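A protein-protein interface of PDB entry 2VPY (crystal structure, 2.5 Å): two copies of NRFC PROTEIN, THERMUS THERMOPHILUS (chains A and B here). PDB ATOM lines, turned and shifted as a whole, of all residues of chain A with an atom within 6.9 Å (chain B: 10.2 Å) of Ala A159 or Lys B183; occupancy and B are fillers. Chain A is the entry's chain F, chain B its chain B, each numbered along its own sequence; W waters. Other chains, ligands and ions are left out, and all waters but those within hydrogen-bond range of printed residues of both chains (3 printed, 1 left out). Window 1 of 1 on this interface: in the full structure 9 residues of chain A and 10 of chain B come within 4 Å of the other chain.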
ATOM      1  N   LYS A 154      30.466  26.331  26.031  1.00  0.00           N
ATOM      2  CA  LYS A 154      29.475  26.121  27.075  1.00  0.00           C
ATOM      3  C   LYS A 154      28.263  27.025  26.909  1.00  0.00           C
ATOM      4  O   LYS A 154      27.132  26.651  27.239  1.00  0.00           O
ATOM      5  CB  LYS A 154      30.091  26.363  28.447  1.00  0.00           C
ATOM      6  CG  LYS A 154      30.944  25.239  28.953  1.00  0.00           C
ATOM      7  CD  LYS A 154      30.970  25.301  30.451  1.00  0.00           C
ATOM      8  CE  LYS A 154      32.024  26.267  30.923  1.00  0.00           C
ATOM      9  NZ  LYS A 154      33.175  25.487  31.462  1.00  0.00           N
ATOM     10  N   ALA A 155      28.515  28.224  26.399  1.00  0.00           N
ATOM     11  CA  ALA A 155      27.475  29.229  26.174  1.00  0.00           C
ATOM     12  C   ALA A 155      26.648  28.859  24.941  1.00  0.00           C
ATOM     13  O   ALA A 155      25.415  28.964  24.954  1.00  0.00           O
ATOM     14  CB  ALA A 155      28.107  30.593  26.016  1.00  0.00           C
ATOM     15  N   LEU A 156      27.328  28.440  23.880  1.00  0.00           N
ATOM     16  CA  LEU A 156      26.627  27.979  22.697  1.00  0.00           C
ATOM     17  C   LEU A 156      25.711  26.847  23.207  1.00  0.00           C
ATOM     18  O   LEU A 156      24.506  26.861  22.946  1.00  0.00           O
ATOM     19  CB  LEU A 156      27.619  27.479  21.635  1.00  0.00           C
ATOM     20  CG  LEU A 156      28.267  28.575  20.769  1.00  0.00           C
ATOM     21  CD1 LEU A 156      29.481  28.022  20.036  1.00  0.00           C
ATOM     22  CD2 LEU A 156      27.259  29.122  19.755  1.00  0.00           C
ATOM     23  N   LYS A 157      26.244  25.895  23.973  1.00  0.00           N
ATOM     24  CA  LYS A 157      25.393  24.816  24.480  1.00  0.00           C
ATOM     25  C   LYS A 157      24.210  25.283  25.315  1.00  0.00           C
ATOM     26  O   LYS A 157      23.135  24.692  25.238  1.00  0.00           O
ATOM     27  CB  LYS A 157      26.166  23.788  25.320  1.00  0.00           C
ATOM     28  CG  LYS A 157      27.029  22.835  24.510  1.00  0.00           C
ATOM     29  CD  LYS A 157      26.214  22.006  23.502  1.00  0.00           C
ATOM     30  CE  LYS A 157      27.128  21.076  22.705  1.00  0.00           C
ATOM     31  NZ  LYS A 157      28.254  20.564  23.565  1.00  0.00           N
ATOM     32  N   ALA A 158      24.384  26.332  26.110  1.00  0.00           N
ATOM     33  CA  ALA A 158      23.293  26.818  26.966  1.00  0.00           C
ATOM     34  C   ALA A 158      22.284  27.748  26.292  1.00  0.00           C
ATOM     35  O   ALA A 158      21.188  27.974  26.816  1.00  0.00           O
ATOM     36  CB  ALA A 158      23.872  27.500  28.222  1.00  0.00           C
ATOM     37  N   ALA A 159      22.639  28.279  25.133  1.00  0.00           N
ATOM     38  CA  ALA A 159      21.749  29.198  24.428  1.00  0.00           C
ATOM     39  C   ALA A 159      20.418  28.583  24.027  1.00  0.00           C
ATOM     40  O   ALA A 159      20.322  27.401  23.712  1.00  0.00           O
ATOM     41  CB  ALA A 159      22.445  29.771  23.174  1.00  0.00           C
ATOM     42  N   GLU A 160      19.397  29.419  24.062  1.00  0.00           N
ATOM     43  CA  GLU A 160      18.056  29.042  23.674  1.00  0.00           C
ATOM     44  C   GLU A 160      18.037  29.143  22.123  1.00  0.00           C
ATOM     45  O   GLU A 160      17.376  28.352  21.452  1.00  0.00           O
ATOM     46  CB  GLU A 160      17.042  30.007  24.328  1.00  0.00           C
ATOM     47  CG  GLU A 160      15.715  29.390  24.844  1.00  0.00           C
ATOM     48  CD  GLU A 160      15.876  28.083  25.673  1.00  0.00           C
ATOM     49  OE1 GLU A 160      16.749  28.029  26.579  1.00  0.00           O
ATOM     50  OE2 GLU A 160      15.109  27.113  25.422  1.00  0.00           O
ATOM     51  N   ARG A 161      18.787  30.093  21.566  1.00  0.00           N
ATOM     52  CA  ARG A 161      18.872  30.282  20.117  1.00  0.00           C
ATOM     53  C   ARG A 161      20.238  30.877  19.705  1.00  0.00           C
ATOM     54  O   ARG A 161      20.858  31.595  20.488  1.00  0.00           O
ATOM     55  CB  ARG A 161      17.712  31.169  19.621  1.00  0.00           C
ATOM     56  CG  ARG A 161      17.686  32.618  20.123  1.00  0.00           C
ATOM     57  CD  ARG A 161      16.590  33.453  19.383  1.00  0.00           C
ATOM     58  NE  ARG A 161      16.745  33.515  17.921  1.00  0.00           N
ATOM     59  CZ  ARG A 161      15.739  33.625  17.051  1.00  0.00           C
ATOM     60  NH1 ARG A 161      14.494  33.684  17.488  1.00  0.00           N
ATOM     61  NH2 ARG A 161      15.962  33.689  15.746  1.00  0.00           N
ATOM     62  N   VAL A 162      20.709  30.569  18.497  1.00  0.00           N
ATOM     63  CA  VAL A 162      22.004  31.049  18.023  1.00  0.00           C
ATOM     64  C   VAL A 162      21.839  31.646  16.630  1.00  0.00           C
ATOM     65  O   VAL A 162      21.226  31.035  15.766  1.00  0.00           O
ATOM     66  CB  VAL A 162      23.042  29.877  17.979  1.00  0.00           C
ATOM     67  CG1 VAL A 162      24.403  30.400  17.571  1.00  0.00           C
ATOM     68  CG2 VAL A 162      23.124  29.195  19.335  1.00  0.00           C
ATOM     69  N   ASP A 163      22.376  32.839  16.421  1.00  0.00           N
ATOM     70  CA  ASP A 163      22.246  33.521  15.147  1.00  0.00           C
ATOM     71  C   ASP A 163      23.569  34.123  14.697  1.00  0.00           C
ATOM     72  O   ASP A 163      24.529  34.243  15.464  1.00  0.00           O
ATOM     73  CB  ASP A 163      21.188  34.633  15.223  1.00  0.00           C
ATOM     74  CG  ASP A 163      19.796  34.131  15.651  1.00  0.00           C
ATOM     75  OD1 ASP A 163      18.903  34.051  14.790  1.00  0.00           O
ATOM     76  OD2 ASP A 163      19.587  33.833  16.851  1.00  0.00           O
ATOM     77  N   TYR A 177      25.682  35.314  18.001  1.00  0.00           N
ATOM     78  CA  TYR A 177      24.809  36.091  18.847  1.00  0.00           C
ATOM     79  C   TYR A 177      23.920  35.128  19.541  1.00  0.00           C
ATOM     80  O   TYR A 177      23.203  34.371  18.897  1.00  0.00           O
ATOM     81  CB  TYR A 177      23.986  37.063  18.024  1.00  0.00           C
ATOM     82  CG  TYR A 177      24.830  38.173  17.478  1.00  0.00           C
ATOM     83  CD1 TYR A 177      25.147  38.232  16.126  1.00  0.00           C
ATOM     84  CD2 TYR A 177      25.327  39.166  18.319  1.00  0.00           C
ATOM     85  CE1 TYR A 177      25.941  39.260  15.613  1.00  0.00           C
ATOM     86  CE2 TYR A 177      26.124  40.204  17.820  1.00  0.00           C
ATOM     87  CZ  TYR A 177      26.425  40.245  16.463  1.00  0.00           C
ATOM     88  OH  TYR A 177      27.186  41.263  15.943  1.00  0.00           O
ATOM     89  N   LEU A 178      23.946  35.133  20.855  1.00  0.00           N
ATOM     90  CA  LEU A 178      23.088  34.181  21.450  1.00  0.00           C
ATOM     91  C   LEU A 178      21.641  34.636  21.498  1.00  0.00           C
ATOM     92  O   LEU A 178      21.090  35.038  20.462  1.00  0.00           O
ATOM     93  CB  LEU A 178      23.674  33.642  22.772  1.00  0.00           C
ATOM     94  CG  LEU A 178      25.092  33.143  22.391  1.00  0.00           C
ATOM     95  CD1 LEU A 178      25.833  32.703  23.627  1.00  0.00           C
ATOM     96  CD2 LEU A 178      25.079  31.997  21.336  1.00  0.00           C
ATOM     97  N   ASN A 179      21.047  34.641  22.670  1.00  0.00           N
ATOM     98  CA  ASN A 179      19.613  34.862  22.775  1.00  0.00           C
ATOM     99  C   ASN A 179      18.914  36.100  22.261  1.00  0.00           C
ATOM    100  O   ASN A 179      18.403  36.885  23.050  1.00  0.00           O
ATOM    101  CB  ASN A 179      19.211  34.560  24.213  1.00  0.00           C
ATOM    102  CG  ASN A 179      19.824  33.263  24.705  1.00  0.00           C
ATOM    103  OD1 ASN A 179      20.689  33.263  25.578  1.00  0.00           O
ATOM    104  ND2 ASN A 179      19.403  32.152  24.116  1.00  0.00           N
ATOM    105  N   VAL B  43      19.770  16.738  12.316  1.00  0.00           N
ATOM    106  CA  VAL B  43      20.854  17.638  12.608  1.00  0.00           C
ATOM    107  C   VAL B  43      21.665  17.144  13.806  1.00  0.00           C
ATOM    108  O   VAL B  43      21.141  17.075  14.908  1.00  0.00           O
ATOM    109  CB  VAL B  43      20.289  19.050  12.991  1.00  0.00           C
ATOM    110  CG1 VAL B  43      21.436  20.054  13.038  1.00  0.00           C
ATOM    111  CG2 VAL B  43      19.193  19.504  12.025  1.00  0.00           C
ATOM    112  N   PRO B  47      24.541  13.204  21.550  1.00  0.00           N
ATOM    113  CA  PRO B  47      24.117  13.942  22.724  1.00  0.00           C
ATOM    114  C   PRO B  47      23.392  15.259  22.496  1.00  0.00           C
ATOM    115  O   PRO B  47      23.145  16.008  23.460  1.00  0.00           O
ATOM    116  CB  PRO B  47      25.443  14.115  23.436  1.00  0.00           C
ATOM    117  CG  PRO B  47      26.441  14.308  22.231  1.00  0.00           C
ATOM    118  CD  PRO B  47      25.645  13.962  20.958  1.00  0.00           C
ATOM    119  N   ASN B  48      23.118  15.520  21.224  1.00  0.00           N
ATOM    120  CA  ASN B  48      22.471  16.740  20.698  1.00  0.00           C
ATOM    121  C   ASN B  48      21.952  16.392  19.278  1.00  0.00           C
ATOM    122  O   ASN B  48      22.469  16.906  18.271  1.00  0.00           O
ATOM    123  CB  ASN B  48      23.480  17.887  20.561  1.00  0.00           C
ATOM    124  CG  ASN B  48      24.463  17.966  21.715  1.00  0.00           C
ATOM    125  OD1 ASN B  48      24.090  17.782  22.869  1.00  0.00           O
ATOM    126  ND2 ASN B  48      25.728  18.272  21.408  1.00  0.00           N
ATOM    127  N   LEU B  49      20.932  15.541  19.238  1.00  0.00           N
ATOM    128  CA  LEU B  49      20.319  15.027  18.019  1.00  0.00           C
ATOM    129  C   LEU B  49      18.927  15.629  17.816  1.00  0.00           C
ATOM    130  O   LEU B  49      17.994  15.318  18.524  1.00  0.00           O
ATOM    131  CB  LEU B  49      20.231  13.484  18.108  1.00  0.00           C
ATOM    132  CG  LEU B  49      20.225  12.629  16.826  1.00  0.00           C
ATOM    133  CD1 LEU B  49      21.162  13.220  15.794  1.00  0.00           C
ATOM    134  CD2 LEU B  49      20.633  11.186  17.145  1.00  0.00           C
ATOM    135  N   VAL B  50      18.810  16.490  16.818  1.00  0.00           N
ATOM    136  CA  VAL B  50      17.543  17.129  16.569  1.00  0.00           C
ATOM    137  C   VAL B  50      16.971  16.663  15.239  1.00  0.00           C
ATOM    138  O   VAL B  50      17.735  16.429  14.300  1.00  0.00           O
ATOM    139  CB  VAL B  50      17.766  18.680  16.554  1.00  0.00           C
ATOM    140  CG1 VAL B  50      16.564  19.399  15.980  1.00  0.00           C
ATOM    141  CG2 VAL B  50      18.099  19.183  17.978  1.00  0.00           C
ATOM    142  N   VAL B  51      15.653  16.469  15.171  1.00  0.00           N
ATOM    143  CA  VAL B  51      15.017  16.137  13.901  1.00  0.00           C
ATOM    144  C   VAL B  51      13.935  17.192  13.611  1.00  0.00           C
ATOM    145  O   VAL B  51      13.114  17.502  14.468  1.00  0.00           O
ATOM    146  CB  VAL B  51      14.376  14.706  13.856  1.00  0.00           C
ATOM    147  CG1 VAL B  51      13.693  14.491  12.489  1.00  0.00           C
ATOM    148  CG2 VAL B  51      15.444  13.624  14.068  1.00  0.00           C
ATOM    149  N   GLU B  52      13.985  17.774  12.413  1.00  0.00           N
ATOM    150  CA  GLU B  52      13.008  18.769  11.964  1.00  0.00           C
ATOM    151  C   GLU B  52      12.135  18.156  10.875  1.00  0.00           C
ATOM    152  O   GLU B  52      12.642  17.649   9.867  1.00  0.00           O
ATOM    153  CB  GLU B  52      13.702  20.030  11.408  1.00  0.00           C
ATOM    154  CG  GLU B  52      12.797  21.075  10.720  1.00  0.00           C
ATOM    155  CD  GLU B  52      13.631  22.094   9.942  1.00  0.00           C
ATOM    156  OE1 GLU B  52      14.095  23.082  10.545  1.00  0.00           O
ATOM    157  OE2 GLU B  52      13.848  21.883   8.730  1.00  0.00           O
ATOM    158  N   GLU B 160       7.648  30.951  20.724  1.00  0.00           N
ATOM    159  CA  GLU B 160       8.985  31.185  21.283  1.00  0.00           C
ATOM    160  C   GLU B 160       9.879  31.775  20.130  1.00  0.00           C
ATOM    161  O   GLU B 160      10.720  32.653  20.361  1.00  0.00           O
ATOM    162  CB  GLU B 160       9.541  29.860  21.819  1.00  0.00           C
ATOM    163  CG  GLU B 160      10.275  29.942  23.160  1.00  0.00           C
ATOM    164  CD  GLU B 160       9.377  30.299  24.354  1.00  0.00           C
ATOM    165  OE1 GLU B 160       8.362  29.589  24.581  1.00  0.00           O
ATOM    166  OE2 GLU B 160       9.697  31.281  25.076  1.00  0.00           O
ATOM    167  N   ARG B 161       9.724  31.283  18.899  1.00  0.00           N
ATOM    168  CA  ARG B 161      10.444  31.868  17.758  1.00  0.00           C
ATOM    169  C   ARG B 161       9.566  31.765  16.516  1.00  0.00           C
ATOM    170  O   ARG B 161       8.661  30.943  16.468  1.00  0.00           O
ATOM    171  CB  ARG B 161      11.810  31.204  17.494  1.00  0.00           C
ATOM    172  CG  ARG B 161      11.797  29.721  17.105  1.00  0.00           C
ATOM    173  CD  ARG B 161      13.229  29.193  17.009  1.00  0.00           C
ATOM    174  NE  ARG B 161      13.951  29.835  15.914  1.00  0.00           N
ATOM    175  CZ  ARG B 161      15.274  29.961  15.823  1.00  0.00           C
ATOM    176  NH1 ARG B 161      16.077  29.488  16.773  1.00  0.00           N
ATOM    177  NH2 ARG B 161      15.791  30.571  14.763  1.00  0.00           N
ATOM    178  N   VAL B 162       9.804  32.629  15.537  1.00  0.00           N
ATOM    179  CA  VAL B 162       9.065  32.605  14.278  1.00  0.00           C
ATOM    180  C   VAL B 162      10.077  32.652  13.104  1.00  0.00           C
ATOM    181  O   VAL B 162      10.990  33.479  13.113  1.00  0.00           O
ATOM    182  CB  VAL B 162       8.063  33.783  14.152  1.00  0.00           C
ATOM    183  CG1 VAL B 162       7.348  33.694  12.816  1.00  0.00           C
ATOM    184  CG2 VAL B 162       7.046  33.743  15.308  1.00  0.00           C
ATOM    185  N   ASP B 163       9.927  31.739  12.134  1.00  0.00           N
ATOM    186  CA  ASP B 163      10.790  31.640  10.945  1.00  0.00           C
ATOM    187  C   ASP B 163      10.030  31.428   9.636  1.00  0.00           C
ATOM    188  O   ASP B 163       8.894  30.944   9.605  1.00  0.00           O
ATOM    189  CB  ASP B 163      11.854  30.543  11.073  1.00  0.00           C
ATOM    190  CG  ASP B 163      12.698  30.680  12.333  1.00  0.00           C
ATOM    191  OD1 ASP B 163      13.762  31.344  12.320  1.00  0.00           O
ATOM    192  OD2 ASP B 163      12.264  30.111  13.352  1.00  0.00           O
ATOM    193  N   ASN B 179       8.436  27.869  16.710  1.00  0.00           N
ATOM    194  CA  ASN B 179       9.295  27.083  17.563  1.00  0.00           C
ATOM    195  C   ASN B 179      10.177  26.001  16.915  1.00  0.00           C
ATOM    196  O   ASN B 179      10.180  24.866  17.371  1.00  0.00           O
ATOM    197  CB  ASN B 179       8.409  26.451  18.635  1.00  0.00           C
ATOM    198  CG  ASN B 179       7.368  27.426  19.186  1.00  0.00           C
ATOM    199  OD1 ASN B 179       6.168  27.117  19.221  1.00  0.00           O
ATOM    200  ND2 ASN B 179       7.821  28.606  19.617  1.00  0.00           N
ATOM    201  N   ALA B 180      10.922  26.347  15.870  1.00  0.00           N
ATOM    202  CA  ALA B 180      11.833  25.411  15.203  1.00  0.00           C
ATOM    203  C   ALA B 180      12.721  24.671  16.213  1.00  0.00           C
ATOM    204  O   ALA B 180      13.302  25.294  17.113  1.00  0.00           O
ATOM    205  CB  ALA B 180      12.720  26.157  14.220  1.00  0.00           C
ATOM    206  N   PRO B 181      12.866  23.337  16.053  1.00  0.00           N
ATOM    207  CA  PRO B 181      13.661  22.426  16.897  1.00  0.00           C
ATOM    208  C   PRO B 181      15.148  22.752  17.037  1.00  0.00           C
ATOM    209  O   PRO B 181      15.713  22.633  18.120  1.00  0.00           O
ATOM    210  CB  PRO B 181      13.439  21.047  16.272  1.00  0.00           C
ATOM    211  CG  PRO B 181      12.969  21.342  14.886  1.00  0.00           C
ATOM    212  CD  PRO B 181      12.163  22.602  14.998  1.00  0.00           C
ATOM    213  N   SER B 182      15.785  23.153  15.944  1.00  0.00           N
ATOM    214  CA  SER B 182      17.202  23.500  15.983  1.00  0.00           C
ATOM    215  C   SER B 182      17.473  24.950  16.423  1.00  0.00           C
ATOM    216  O   SER B 182      16.825  25.859  15.920  1.00  0.00           O
ATOM    217  CB  SER B 182      17.850  23.273  14.620  1.00  0.00           C
ATOM    218  OG  SER B 182      19.208  23.652  14.689  1.00  0.00           O
ATOM    219  N   LYS B 183      18.432  25.165  17.335  1.00  0.00           N
ATOM    220  CA  LYS B 183      18.777  26.514  17.846  1.00  0.00           C
ATOM    221  C   LYS B 183      19.142  27.529  16.777  1.00  0.00           C
ATOM    222  O   LYS B 183      18.941  28.727  16.948  1.00  0.00           O
ATOM    223  CB  LYS B 183      19.986  26.492  18.770  1.00  0.00           C
ATOM    224  CG  LYS B 183      19.812  25.947  20.130  1.00  0.00           C
ATOM    225  CD  LYS B 183      21.167  25.968  20.780  1.00  0.00           C
ATOM    226  CE  LYS B 183      21.276  24.824  21.734  1.00  0.00           C
ATOM    227  NZ  LYS B 183      21.888  25.193  23.046  1.00  0.00           N
ATOM    228  N   LYS B 184      19.731  27.028  15.699  1.00  0.00           N
ATOM    229  CA  LYS B 184      20.176  27.837  14.565  1.00  0.00           C
ATOM    230  C   LYS B 184      19.079  28.116  13.568  1.00  0.00           C
ATOM    231  O   LYS B 184      19.302  28.769  12.558  1.00  0.00           O
ATOM    232  CB  LYS B 184      21.332  27.147  13.850  1.00  0.00           C
ATOM    233  CG  LYS B 184      22.557  27.016  14.698  1.00  0.00           C
ATOM    234  CD  LYS B 184      23.472  25.978  14.103  1.00  0.00           C
ATOM    235  CE  LYS B 184      24.794  25.908  14.852  1.00  0.00           C
ATOM    236  NZ  LYS B 184      25.639  27.138  14.653  1.00  0.00           N
ATOM    237  N   GLY B 185      17.903  27.580  13.839  1.00  0.00           N
ATOM    238  CA  GLY B 185      16.777  27.826  12.960  1.00  0.00           C
ATOM    239  C   GLY B 185      16.426  26.788  11.915  1.00  0.00           C
ATOM    240  O   GLY B 185      16.869  25.637  11.974  1.00  0.00           O
ATOM    241  N   LEU B 186      15.608  27.192  10.957  1.00  0.00           N
ATOM    242  CA  LEU B 186      15.214  26.272   9.922  1.00  0.00           C
ATOM    243  C   LEU B 186      16.462  25.722   9.248  1.00  0.00           C
ATOM    244  O   LEU B 186      17.452  26.409   9.020  1.00  0.00           O
ATOM    245  CB  LEU B 186      14.284  26.947   8.902  1.00  0.00           C
ATOM    246  CG  LEU B 186      12.991  27.507   9.552  1.00  0.00           C
ATOM    247  CD1 LEU B 186      12.189  28.325   8.552  1.00  0.00           C
ATOM    248  CD2 LEU B 186      12.128  26.378  10.100  1.00  0.00           C
ATOM    249  N   THR B 187      16.399  24.440   8.995  1.00  0.00           N
ATOM    250  CA  THR B 187      17.414  23.648   8.354  1.00  0.00           C
ATOM    251  C   THR B 187      17.629  24.014   6.837  1.00  0.00           C
ATOM    252  O   THR B 187      16.665  24.245   6.134  1.00  0.00           O
ATOM    253  CB  THR B 187      16.906  22.216   8.533  1.00  0.00           C
ATOM    254  OG1 THR B 187      17.682  21.528   9.509  1.00  0.00           O
ATOM    255  CG2 THR B 187      16.830  21.533   7.272  1.00  0.00           C
HETATM  256  O   HOH W   1      13.593  33.440  14.348  1.00  0.00           O
HETATM  257  O   HOH W   2      13.209  33.503  19.833  1.00  0.00           O
HETATM  258  O   HOH W   3      15.541  28.327  19.480  1.00  0.00           O
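Asn B48 touches Lys A157.
Lys B183 touches Glu A160 (CG to O, 3.7 Å).
Arg A161 touches Lys B183.
Val A162 touches Lys B184.
Arg B161 touches its own counterpart, Arg A161.
Positions printed for both chains: 160, 161, 162, 163 and 179.
The backbone carbonyl oxygen of Leu A156 sits at hydrogen-bond distance from the side-chain amino group of Lys B183 (3.1 Å).
O of Lys A157 is in hydrogen-bond range of NZ of Lys B183 (2.6 Å).
The side-chain amino group (NZ) of Lys B183 sits at hydrogen-bond distance from the backbone carbonyl oxygen (O) of Ala A159, 2.8 Å away.
N of Val A162 lies within hydrogen-bond range of O of Lys B183.
NH2 of Arg A161 sits close to NH2 of Arg B161 (3.3 Å).
Of the 20 printed residues of chain B, 4 touch a printed residue of chain A.
Printed residues of chain B that touch a printed residue of chain A: Asn B48, Arg B161, Lys B183 and Lys B184.
Among the printed residues, no Asp or Glu carboxylate lies within 4 Å of a Lys or Arg side-chain nitrogen of the other chain.
No residue of chain B comes within 4 Å of Ala A155.
Of the printed residues of chain B, Leu A156 touches Lys B183 (3.1 Å).
Of the printed residues of chain B, Lys A157 touches Asn B48 and Lys B183.
No residue of chain B comes within 4 Å of Ala A158.
Ala A159 touches one residue of chain B.
Of the printed residues of chain B, Arg A161 touches Arg B161 and Lys B183.
Val A162 touches just these residues of chain B: Lys B183 and Lys B184.
No residue of chain B comes within 4 Å of Leu A178.
Val B51 touches none of the printed residues of chain A.
Of the printed residues of chain A, Arg B161 touches Arg A161.
Ser B182 touches none of the printed residues of chain A.
Printed residues of chain A within 4 Å of Lys B183: Leu A156 (3.1 Å), Lys A157 (2.6 Å), Ala A159 (2.8 Å), Glu A160 (3.7 Å), Arg A161 (3.5 Å) and Val A162 (3.0 Å).
Printed residues of chain A within 4 Å of Lys B184: Val A162 (3.6 Å).
The nearest residue of chain B that does not touch Ala A159 is Lys B184 (8.0 Å).
The guanidinium group of Arg B161 is in salt-bridge range of the side-chain carboxylate of Asp B163 (3.1 Å).
The backbone NH (N) of Asn B179 lies within hydrogen-bond range of the backbone carbonyl oxygen (O) of Arg B161 (3.1 Å).
NH1 of Arg B161 is in hydrogen-bond range of O of Lys B183.
N of Glu A160 lies close to ND2 of Asn A179, 2.7 Å away.
OD2 of Asp A163 lies within salt-bridge range of NE of Arg A161 (3.1 Å).
N of Arg A161 lies close to ND2 of Asn A179, at 3.3 Å.
Water W2 bridges NH1 of Arg A161 (2.7 Å) and O of Glu B160 (2.7 Å).
Water W3 bridges the backbone carbonyl oxygen (O) of Glu A160 (2.7 Å) and the guanidinium group (NH1) of Arg B161 (3.0 Å).
Water W1 lies within hydrogen-bond range of NH2 of Arg A161, O of Val B162 and OD1 of Asp B163.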
